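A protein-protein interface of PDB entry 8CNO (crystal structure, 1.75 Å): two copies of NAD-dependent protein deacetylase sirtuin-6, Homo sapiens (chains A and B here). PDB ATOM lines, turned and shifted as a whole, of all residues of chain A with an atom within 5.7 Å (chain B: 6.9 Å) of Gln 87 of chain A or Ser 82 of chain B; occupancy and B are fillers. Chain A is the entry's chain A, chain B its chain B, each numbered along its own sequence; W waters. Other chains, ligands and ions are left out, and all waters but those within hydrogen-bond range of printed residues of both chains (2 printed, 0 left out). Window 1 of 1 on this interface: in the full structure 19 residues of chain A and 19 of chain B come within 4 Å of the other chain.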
ATOM      1  N   ARG A  84       2.234 -14.186 -23.313  1.00  0.00           N
ATOM      2  CA  ARG A  84       2.450 -14.227 -21.844  1.00  0.00           C
ATOM      3  C   ARG A  84       2.295 -15.671 -21.375  1.00  0.00           C
ATOM      4  O   ARG A  84       1.456 -16.424 -21.923  1.00  0.00           O
ATOM      5  CB  ARG A  84       1.617 -13.159 -21.130  1.00  0.00           C
ATOM      6  CG  ARG A  84       0.107 -13.218 -21.267  1.00  0.00           C
ATOM      7  CD  ARG A  84      -0.471 -12.604 -19.992  1.00  0.00           C
ATOM      8  NE  ARG A  84      -0.159 -13.491 -18.884  1.00  0.00           N
ATOM      9  CZ  ARG A  84       0.254 -13.153 -17.665  1.00  0.00           C
ATOM     10  NH1 ARG A  84       0.450 -11.888 -17.327  1.00  0.00           N
ATOM     11  NH2 ARG A  84       0.516 -14.110 -16.791  1.00  0.00           N
ATOM     12  N   PRO A  85       3.124 -16.143 -20.407  1.00  0.00           N
ATOM     13  CA  PRO A  85       2.892 -17.435 -19.757  1.00  0.00           C
ATOM     14  C   PRO A  85       1.456 -17.477 -19.221  1.00  0.00           C
ATOM     15  O   PRO A  85       0.954 -16.519 -18.656  1.00  0.00           O
ATOM     16  CB  PRO A  85       3.919 -17.502 -18.601  1.00  0.00           C
ATOM     17  CG  PRO A  85       4.974 -16.475 -18.990  1.00  0.00           C
ATOM     18  CD  PRO A  85       4.225 -15.412 -19.769  1.00  0.00           C
ATOM     19  N   THR A  86       0.796 -18.613 -19.431  1.00  0.00           N
ATOM     20  CA  THR A  86      -0.543 -18.932 -18.894  1.00  0.00           C
ATOM     21  C   THR A  86      -0.484 -19.114 -17.380  1.00  0.00           C
ATOM     22  O   THR A  86       0.642 -19.282 -16.816  1.00  0.00           O
ATOM     23  CB  THR A  86      -1.103 -20.190 -19.559  1.00  0.00           C
ATOM     24  OG1 THR A  86      -0.315 -21.309 -19.120  1.00  0.00           O
ATOM     25  CG2 THR A  86      -1.069 -20.079 -21.053  1.00  0.00           C
ATOM     26  N   GLN A  87      -1.666 -19.178 -16.783  1.00  0.00           N
ATOM     27  CA  GLN A  87      -1.879 -19.584 -15.367  1.00  0.00           C
ATOM     28  C   GLN A  87      -1.147 -20.924 -15.163  1.00  0.00           C
ATOM     29  O   GLN A  87      -0.422 -21.025 -14.166  1.00  0.00           O
ATOM     30  CB  GLN A  87      -3.362 -19.566 -15.049  1.00  0.00           C
ATOM     31  CG  GLN A  87      -3.963 -18.173 -15.198  1.00  0.00           C
ATOM     32  CD  GLN A  87      -5.472 -18.262 -15.204  1.00  0.00           C
ATOM     33  OE1 GLN A  87      -6.124 -18.172 -14.165  1.00  0.00           O
ATOM     34  NE2 GLN A  87      -6.035 -18.494 -16.374  1.00  0.00           N
ATOM     35  N   THR A  88      -1.288 -21.880 -16.093  1.00  0.00           N
ATOM     36  CA  THR A  88      -0.580 -23.191 -16.018  1.00  0.00           C
ATOM     37  C   THR A  88       0.932 -22.953 -15.951  1.00  0.00           C
ATOM     38  O   THR A  88       1.571 -23.586 -15.030  1.00  0.00           O
ATOM     39  CB  THR A  88      -0.986 -24.163 -17.146  1.00  0.00           C
ATOM     40  OG1 THR A  88      -2.347 -24.496 -16.923  1.00  0.00           O
ATOM     41  CG2 THR A  88      -0.194 -25.455 -17.054  1.00  0.00           C
ATOM     42  N   HIS A  89       1.544 -22.155 -16.850  1.00  0.00           N
ATOM     43  CA  HIS A  89       3.012 -21.925 -16.805  1.00  0.00           C
ATOM     44  C   HIS A  89       3.430 -21.425 -15.421  1.00  0.00           C
ATOM     45  O   HIS A  89       4.397 -21.903 -14.871  1.00  0.00           O
ATOM     46  CB  HIS A  89       3.456 -20.933 -17.868  1.00  0.00           C
ATOM     47  CG  HIS A  89       3.415 -21.460 -19.255  1.00  0.00           C
ATOM     48  ND1 HIS A  89       2.350 -21.235 -20.071  1.00  0.00           N
ATOM     49  CD2 HIS A  89       4.338 -22.142 -19.979  1.00  0.00           C
ATOM     50  CE1 HIS A  89       2.557 -21.805 -21.239  1.00  0.00           C
ATOM     51  NE2 HIS A  89       3.788 -22.413 -21.184  1.00  0.00           N
ATOM     52  N   MET A  90       2.719 -20.437 -14.917  1.00  0.00           N
ATOM     53  CA  MET A  90       3.059 -19.793 -13.624  1.00  0.00           C
ATOM     54  C   MET A  90       2.774 -20.745 -12.454  1.00  0.00           C
ATOM     55  O   MET A  90       3.502 -20.648 -11.452  1.00  0.00           O
ATOM     56  CB  MET A  90       2.251 -18.493 -13.521  1.00  0.00           C
ATOM     57  CG  MET A  90       2.669 -17.433 -14.518  1.00  0.00           C
ATOM     58  SD  MET A  90       4.453 -17.261 -14.889  1.00  0.00           S
ATOM     59  CE  MET A  90       5.113 -16.740 -13.317  1.00  0.00           C
ATOM     60  N   ALA A  91       1.792 -21.664 -12.550  1.00  0.00           N
ATOM     61  CA  ALA A  91       1.524 -22.638 -11.479  1.00  0.00           C
ATOM     62  C   ALA A  91       2.769 -23.528 -11.357  1.00  0.00           C
ATOM     63  O   ALA A  91       3.143 -23.856 -10.228  1.00  0.00           O
ATOM     64  CB  ALA A  91       0.280 -23.451 -11.739  1.00  0.00           C
ATOM     65  N   LEU A  92       3.323 -23.917 -12.489  1.00  0.00           N
ATOM     66  CA  LEU A  92       4.499 -24.838 -12.561  1.00  0.00           C
ATOM     67  C   LEU A  92       5.707 -24.134 -11.912  1.00  0.00           C
ATOM     68  O   LEU A  92       6.480 -24.820 -11.226  1.00  0.00           O
ATOM     69  CB  LEU A  92       4.788 -25.184 -14.020  1.00  0.00           C
ATOM     70  CG  LEU A  92       3.752 -26.082 -14.674  1.00  0.00           C
ATOM     71  CD1 LEU A  92       4.004 -26.248 -16.165  1.00  0.00           C
ATOM     72  CD2 LEU A  92       3.632 -27.396 -13.911  1.00  0.00           C
ATOM     73  N   ASP A 253      -5.746 -24.796 -17.577  1.00  0.00           N
ATOM     74  CA  ASP A 253      -5.799 -23.618 -16.654  1.00  0.00           C
ATOM     75  C   ASP A 253      -6.840 -23.859 -15.536  1.00  0.00           C
ATOM     76  O   ASP A 253      -6.546 -23.519 -14.385  1.00  0.00           O
ATOM     77  CB  ASP A 253      -6.060 -22.319 -17.415  1.00  0.00           C
ATOM     78  CG  ASP A 253      -4.818 -21.727 -18.060  1.00  0.00           C
ATOM     79  OD1 ASP A 253      -3.684 -22.251 -17.787  1.00  0.00           O
ATOM     80  OD2 ASP A 253      -4.983 -20.779 -18.874  1.00  0.00           O
ATOM     81  N   GLU A 254      -8.031 -24.369 -15.858  1.00  0.00           N
ATOM     82  CA  GLU A 254      -9.063 -24.734 -14.848  1.00  0.00           C
ATOM     83  C   GLU A 254      -8.461 -25.769 -13.910  1.00  0.00           C
ATOM     84  O   GLU A 254      -8.512 -25.602 -12.676  1.00  0.00           O
ATOM     85  CB  GLU A 254     -10.339 -25.242 -15.521  1.00  0.00           C
ATOM     86  CG  GLU A 254     -11.395 -25.537 -14.493  1.00  0.00           C
ATOM     87  CD  GLU A 254     -12.808 -25.763 -14.987  1.00  0.00           C
ATOM     88  OE1 GLU A 254     -13.698 -25.821 -14.123  1.00  0.00           O
ATOM     89  OE2 GLU A 254     -13.003 -25.912 -16.206  1.00  0.00           O
ATOM     90  N   MET A 256      -5.288 -26.677 -13.247  1.00  0.00           N
ATOM     91  CA  MET A 256      -4.116 -26.172 -12.474  1.00  0.00           C
ATOM     92  C   MET A 256      -4.572 -25.094 -11.478  1.00  0.00           C
ATOM     93  O   MET A 256      -4.096 -25.120 -10.312  1.00  0.00           O
ATOM     94  CB  MET A 256      -3.054 -25.681 -13.469  1.00  0.00           C
ATOM     95  CG  MET A 256      -2.368 -26.798 -14.242  1.00  0.00           C
ATOM     96  SD  MET A 256      -1.576 -28.084 -13.264  1.00  0.00           S
ATOM     97  CE  MET A 256      -0.368 -27.125 -12.355  1.00  0.00           C
ATOM     98  N   THR A 257      -5.594 -24.267 -11.757  1.00  0.00           N
ATOM     99  CA  THR A 257      -6.010 -23.257 -10.746  1.00  0.00           C
ATOM    100  C   THR A 257      -6.669 -23.975  -9.565  1.00  0.00           C
ATOM    101  O   THR A 257      -6.420 -23.589  -8.434  1.00  0.00           O
ATOM    102  CB  THR A 257      -6.886 -22.145 -11.355  1.00  0.00           C
ATOM    103  OG1 THR A 257      -7.947 -22.731 -12.081  1.00  0.00           O
ATOM    104  CG2 THR A 257      -6.115 -21.272 -12.316  1.00  0.00           C
ATOM    105  N   ILE A 267      -0.837 -18.498  -7.296  1.00  0.00           N
ATOM    106  CA  ILE A 267      -0.168 -18.504  -8.624  1.00  0.00           C
ATOM    107  C   ILE A 267       0.555 -17.163  -8.717  1.00  0.00           C
ATOM    108  O   ILE A 267      -0.070 -16.089  -8.624  1.00  0.00           O
ATOM    109  CB  ILE A 267      -1.149 -18.790  -9.775  1.00  0.00           C
ATOM    110  CG1 ILE A 267      -1.699 -20.226  -9.733  1.00  0.00           C
ATOM    111  CG2 ILE A 267      -0.468 -18.494 -11.098  1.00  0.00           C
ATOM    112  CD1 ILE A 267      -2.733 -20.546 -10.790  1.00  0.00           C
ATOM    113  N   SER B  53      -6.322 -14.428 -24.758  1.00  0.00           N
ATOM    114  CA  SER B  53      -6.722 -15.245 -23.579  1.00  0.00           C
ATOM    115  C   SER B  53      -7.482 -16.518 -23.972  1.00  0.00           C
ATOM    116  O   SER B  53      -7.951 -17.239 -23.069  1.00  0.00           O
ATOM    117  CB  SER B  53      -7.488 -14.384 -22.618  1.00  0.00           C
ATOM    118  OG  SER B  53      -6.565 -13.611 -21.869  1.00  0.00           O
ATOM    119  N   THR B  78     -10.218 -21.465 -23.403  1.00  0.00           N
ATOM    120  CA  THR B  78     -10.576 -21.183 -21.987  1.00  0.00           C
ATOM    121  C   THR B  78     -12.093 -21.263 -21.831  1.00  0.00           C
ATOM    122  O   THR B  78     -12.783 -21.091 -22.840  1.00  0.00           O
ATOM    123  CB  THR B  78     -10.091 -19.783 -21.595  1.00  0.00           C
ATOM    124  OG1 THR B  78     -10.142 -19.645 -20.180  1.00  0.00           O
ATOM    125  CG2 THR B  78     -10.915 -18.683 -22.246  1.00  0.00           C
ATOM    126  N   THR B  79     -12.591 -21.470 -20.616  1.00  0.00           N
ATOM    127  CA  THR B  79     -13.990 -21.102 -20.284  1.00  0.00           C
ATOM    128  C   THR B  79     -14.017 -19.615 -19.966  1.00  0.00           C
ATOM    129  O   THR B  79     -12.910 -18.977 -19.744  1.00  0.00           O
ATOM    130  CB  THR B  79     -14.537 -21.903 -19.101  1.00  0.00           C
ATOM    131  OG1 THR B  79     -13.667 -21.590 -18.014  1.00  0.00           O
ATOM    132  CG2 THR B  79     -14.595 -23.390 -19.385  1.00  0.00           C
ATOM    133  N   PHE B  80     -15.207 -19.020 -19.921  1.00  0.00           N
ATOM    134  CA  PHE B  80     -15.299 -17.594 -19.524  1.00  0.00           C
ATOM    135  C   PHE B  80     -14.753 -17.433 -18.100  1.00  0.00           C
ATOM    136  O   PHE B  80     -14.076 -16.430 -17.812  1.00  0.00           O
ATOM    137  CB  PHE B  80     -16.731 -17.085 -19.725  1.00  0.00           C
ATOM    138  CG  PHE B  80     -17.057 -16.898 -21.187  1.00  0.00           C
ATOM    139  CD1 PHE B  80     -16.423 -15.917 -21.935  1.00  0.00           C
ATOM    140  CD2 PHE B  80     -17.956 -17.746 -21.825  1.00  0.00           C
ATOM    141  CE1 PHE B  80     -16.696 -15.772 -23.287  1.00  0.00           C
ATOM    142  CE2 PHE B  80     -18.232 -17.595 -23.175  1.00  0.00           C
ATOM    143  CZ  PHE B  80     -17.608 -16.613 -23.904  1.00  0.00           C
ATOM    144  N   GLU B  81     -15.051 -18.391 -17.229  1.00  0.00           N
ATOM    145  CA  GLU B  81     -14.644 -18.315 -15.800  1.00  0.00           C
ATOM    146  C   GLU B  81     -13.121 -18.418 -15.619  1.00  0.00           C
ATOM    147  O   GLU B  81     -12.600 -17.813 -14.649  1.00  0.00           O
ATOM    148  CB  GLU B  81     -15.363 -19.408 -15.022  1.00  0.00           C
ATOM    149  CG  GLU B  81     -16.855 -19.144 -14.889  1.00  0.00           C
ATOM    150  CD  GLU B  81     -17.751 -19.708 -15.973  1.00  0.00           C
ATOM    151  OE1 GLU B  81     -17.216 -20.126 -17.045  1.00  0.00           O
ATOM    152  OE2 GLU B  81     -19.002 -19.721 -15.744  1.00  0.00           O
ATOM    153  N   SER B  82     -12.434 -19.187 -16.461  1.00  0.00           N
ATOM    154  CA  SER B  82     -10.989 -19.507 -16.331  1.00  0.00           C
ATOM    155  C   SER B  82     -10.145 -18.573 -17.218  1.00  0.00           C
ATOM    156  O   SER B  82      -8.925 -18.712 -17.150  1.00  0.00           O
ATOM    157  CB  SER B  82     -10.707 -20.952 -16.638  1.00  0.00           C
ATOM    158  OG  SER B  82     -11.326 -21.806 -15.676  1.00  0.00           O
ATOM    159  N   ALA B  83     -10.761 -17.647 -17.970  1.00  0.00           N
ATOM    160  CA  ALA B  83     -10.055 -16.669 -18.842  1.00  0.00           C
ATOM    161  C   ALA B  83      -9.267 -15.741 -17.910  1.00  0.00           C
ATOM    162  O   ALA B  83      -9.807 -15.353 -16.849  1.00  0.00           O
ATOM    163  CB  ALA B  83     -11.005 -15.884 -19.713  1.00  0.00           C
ATOM    164  N   ARG B  84      -8.037 -15.388 -18.269  1.00  0.00           N
ATOM    165  CA  ARG B  84      -7.338 -14.322 -17.504  1.00  0.00           C
ATOM    166  C   ARG B  84      -7.337 -13.060 -18.363  1.00  0.00           C
ATOM    167  O   ARG B  84      -7.316 -13.173 -19.608  1.00  0.00           O
ATOM    168  CB  ARG B  84      -5.973 -14.800 -17.002  1.00  0.00           C
ATOM    169  CG  ARG B  84      -4.978 -15.202 -18.071  1.00  0.00           C
ATOM    170  CD  ARG B  84      -3.566 -14.977 -17.552  1.00  0.00           C
ATOM    171  NE  ARG B  84      -3.351 -13.538 -17.403  1.00  0.00           N
ATOM    172  CZ  ARG B  84      -2.915 -12.901 -16.311  1.00  0.00           C
ATOM    173  NH1 ARG B  84      -2.561 -13.562 -15.222  1.00  0.00           N
ATOM    174  NH2 ARG B  84      -2.813 -11.580 -16.325  1.00  0.00           N
ATOM    175  N   LEU B 112     -14.272  -9.679 -18.775  1.00  0.00           N
ATOM    176  CA  LEU B 112     -12.816  -9.566 -18.435  1.00  0.00           C
ATOM    177  C   LEU B 112     -12.460  -8.169 -17.911  1.00  0.00           C
ATOM    178  O   LEU B 112     -11.720  -8.084 -16.936  1.00  0.00           O
ATOM    179  CB  LEU B 112     -11.985  -9.975 -19.662  1.00  0.00           C
ATOM    180  CG  LEU B 112     -11.915 -11.496 -19.843  1.00  0.00           C
ATOM    181  CD1 LEU B 112     -11.181 -11.897 -21.113  1.00  0.00           C
ATOM    182  CD2 LEU B 112     -11.270 -12.159 -18.629  1.00  0.00           C
ATOM    183  N   ARG B 115     -13.633  -8.201 -14.211  1.00  0.00           N
ATOM    184  CA  ARG B 115     -12.828  -9.176 -13.421  1.00  0.00           C
ATOM    185  C   ARG B 115     -11.357  -8.732 -13.331  1.00  0.00           C
ATOM    186  O   ARG B 115     -10.626  -9.199 -12.402  1.00  0.00           O
ATOM    187  CB  ARG B 115     -13.000 -10.576 -13.986  1.00  0.00           C
ATOM    188  CG  ARG B 115     -14.372 -11.189 -13.748  1.00  0.00           C
ATOM    189  CD  ARG B 115     -14.714 -12.275 -14.727  1.00  0.00           C
ATOM    190  NE  ARG B 115     -14.091 -13.546 -14.397  1.00  0.00           N
ATOM    191  CZ  ARG B 115     -14.496 -14.386 -13.454  1.00  0.00           C
ATOM    192  NH1 ARG B 115     -15.498 -14.065 -12.646  1.00  0.00           N
ATOM    193  NH2 ARG B 115     -13.837 -15.515 -13.276  1.00  0.00           N
ATOM    194  N   PHE B 131     -21.468 -12.354 -16.777  1.00  0.00           N
ATOM    195  CA  PHE B 131     -21.458 -12.615 -15.315  1.00  0.00           C
ATOM    196  C   PHE B 131     -22.456 -11.728 -14.560  1.00  0.00           C
ATOM    197  O   PHE B 131     -22.634 -11.924 -13.324  1.00  0.00           O
ATOM    198  CB  PHE B 131     -20.060 -12.412 -14.729  1.00  0.00           C
ATOM    199  CG  PHE B 131     -19.007 -13.333 -15.291  1.00  0.00           C
ATOM    200  CD1 PHE B 131     -18.498 -13.119 -16.569  1.00  0.00           C
ATOM    201  CD2 PHE B 131     -18.544 -14.412 -14.559  1.00  0.00           C
ATOM    202  CE1 PHE B 131     -17.529 -13.964 -17.088  1.00  0.00           C
ATOM    203  CE2 PHE B 131     -17.519 -15.211 -15.055  1.00  0.00           C
ATOM    204  CZ  PHE B 131     -17.017 -14.966 -16.325  1.00  0.00           C
ATOM    205  N   TRP B 270      -2.408  -9.128 -11.846  1.00  0.00           N
ATOM    206  CA  TRP B 270      -3.826  -9.529 -11.670  1.00  0.00           C
ATOM    207  C   TRP B 270      -3.923 -10.461 -10.463  1.00  0.00           C
ATOM    208  O   TRP B 270      -3.406 -11.590 -10.546  1.00  0.00           O
ATOM    209  CB  TRP B 270      -4.386 -10.175 -12.944  1.00  0.00           C
ATOM    210  CG  TRP B 270      -5.844 -10.505 -12.873  1.00  0.00           C
ATOM    211  CD1 TRP B 270      -6.881  -9.634 -12.641  1.00  0.00           C
ATOM    212  CD2 TRP B 270      -6.442 -11.805 -13.023  1.00  0.00           C
ATOM    213  NE1 TRP B 270      -8.073 -10.308 -12.650  1.00  0.00           N
ATOM    214  CE2 TRP B 270      -7.835 -11.631 -12.911  1.00  0.00           C
ATOM    215  CE3 TRP B 270      -5.943 -13.096 -13.269  1.00  0.00           C
ATOM    216  CZ2 TRP B 270      -8.726 -12.697 -12.997  1.00  0.00           C
ATOM    217  CZ3 TRP B 270      -6.824 -14.151 -13.334  1.00  0.00           C
ATOM    218  CH2 TRP B 270      -8.203 -13.950 -13.219  1.00  0.00           C
HETATM  219  O   HOH W   1      -7.329 -19.722 -19.353  1.00  0.00           O
HETATM  220  O   HOH W   2     -13.606 -22.990 -15.948  1.00  0.00           O
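The backbone carbonyl oxygen (O) of Ser 82 of chain B lies within hydrogen-bond range of the side-chain amide nitrogen (NE2) of Gln 87 of chain A, at 3.0 Å.
The guanidinium group of Arg 84 of chain A lies close to the guanidinium group of Arg 84 of chain B (3.4 Å).
The backbone carbonyl oxygen of Glu 254 of chain A sits at hydrogen-bond distance from the side-chain hydroxyl of Thr 257 of chain A, 3.0 Å away.
The side-chain hydroxyl (OG) of Ser 53 of chain B lies within hydrogen-bond range of the backbone carbonyl oxygen (O) of Arg 84 of chain B (2.4 Å).
O of Ser 82 of chain B sits close to OG1 of Thr 78 of chain B (3.4 Å).
N of Ser 82 of chain B is in hydrogen-bond range of OG1 of Thr 79 of chain B (3.1 Å).
Arg 84 of chain B touches Gln 87 of chain A (CB to NE2, 3.7 Å).
OG of Ser 82 of chain B touches CB of Glu 254 of chain A, at 3.6 Å.
Of chain B, only Ser 82 (3.0 Å) and Arg 84 (3.7 Å) come within 4 Å of Gln 87 of chain A.
Of the printed residues of chain A, Arg 84 of chain B touches Arg 84 (3.4 Å) and Gln 87 (3.7 Å).
Printed residues of chain B within 4 Å of Glu 254 of chain A: Ser 82 (3.6 Å).
Of the printed residues of chain B, Arg 84 of chain A touches Arg 84.
Thr 79 of chain B touches none of the printed residues of chain A.
The nearest residue of chain B that does not touch Gln 87 of chain A is Trp 270 of chain B (4.2 Å).
The nearest residue of chain A that does not touch Ser 82 of chain B is Asp 253 of chain A (4.6 Å).
The nearest printed residue of chain B that does not touch Glu 254 of chain A is Thr 79 of chain B (4.4 Å).
Of the 14 printed residues of chain A, 3 touch a printed residue of chain B.
Printed residues of chain A that touch a printed residue of chain B: Arg 84, Gln 87 and Glu 254.
Printed residues of chain B that touch a printed residue of chain A: Ser 82 and Arg 84.
Arg 84 of chain B touches its own counterpart, Arg 84 of chain A.
Of the 4 pairs that touch across the chains among the printed residues, 1 has its exchanged pair printed and touching as well.
Water W2 lies within hydrogen-bond range of the side-chain hydroxyl of Thr 79 of chain B (2.5 Å), the side-chain hydroxyl of Ser 82 of chain B (2.6 Å) and the side-chain carboxylate of Glu 254 of chain A (3.0 Å).
Water W1 lies within hydrogen-bond range of the side-chain carboxylate of Asp 253 of chain A (2.6 Å), the backbone carbonyl oxygen of Ser 82 of chain B (2.9 Å), the side-chain hydroxyl of Thr 78 of chain B (2.9 Å) and the side-chain amide nitrogen of Gln 87 of chain A (3.5 Å).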
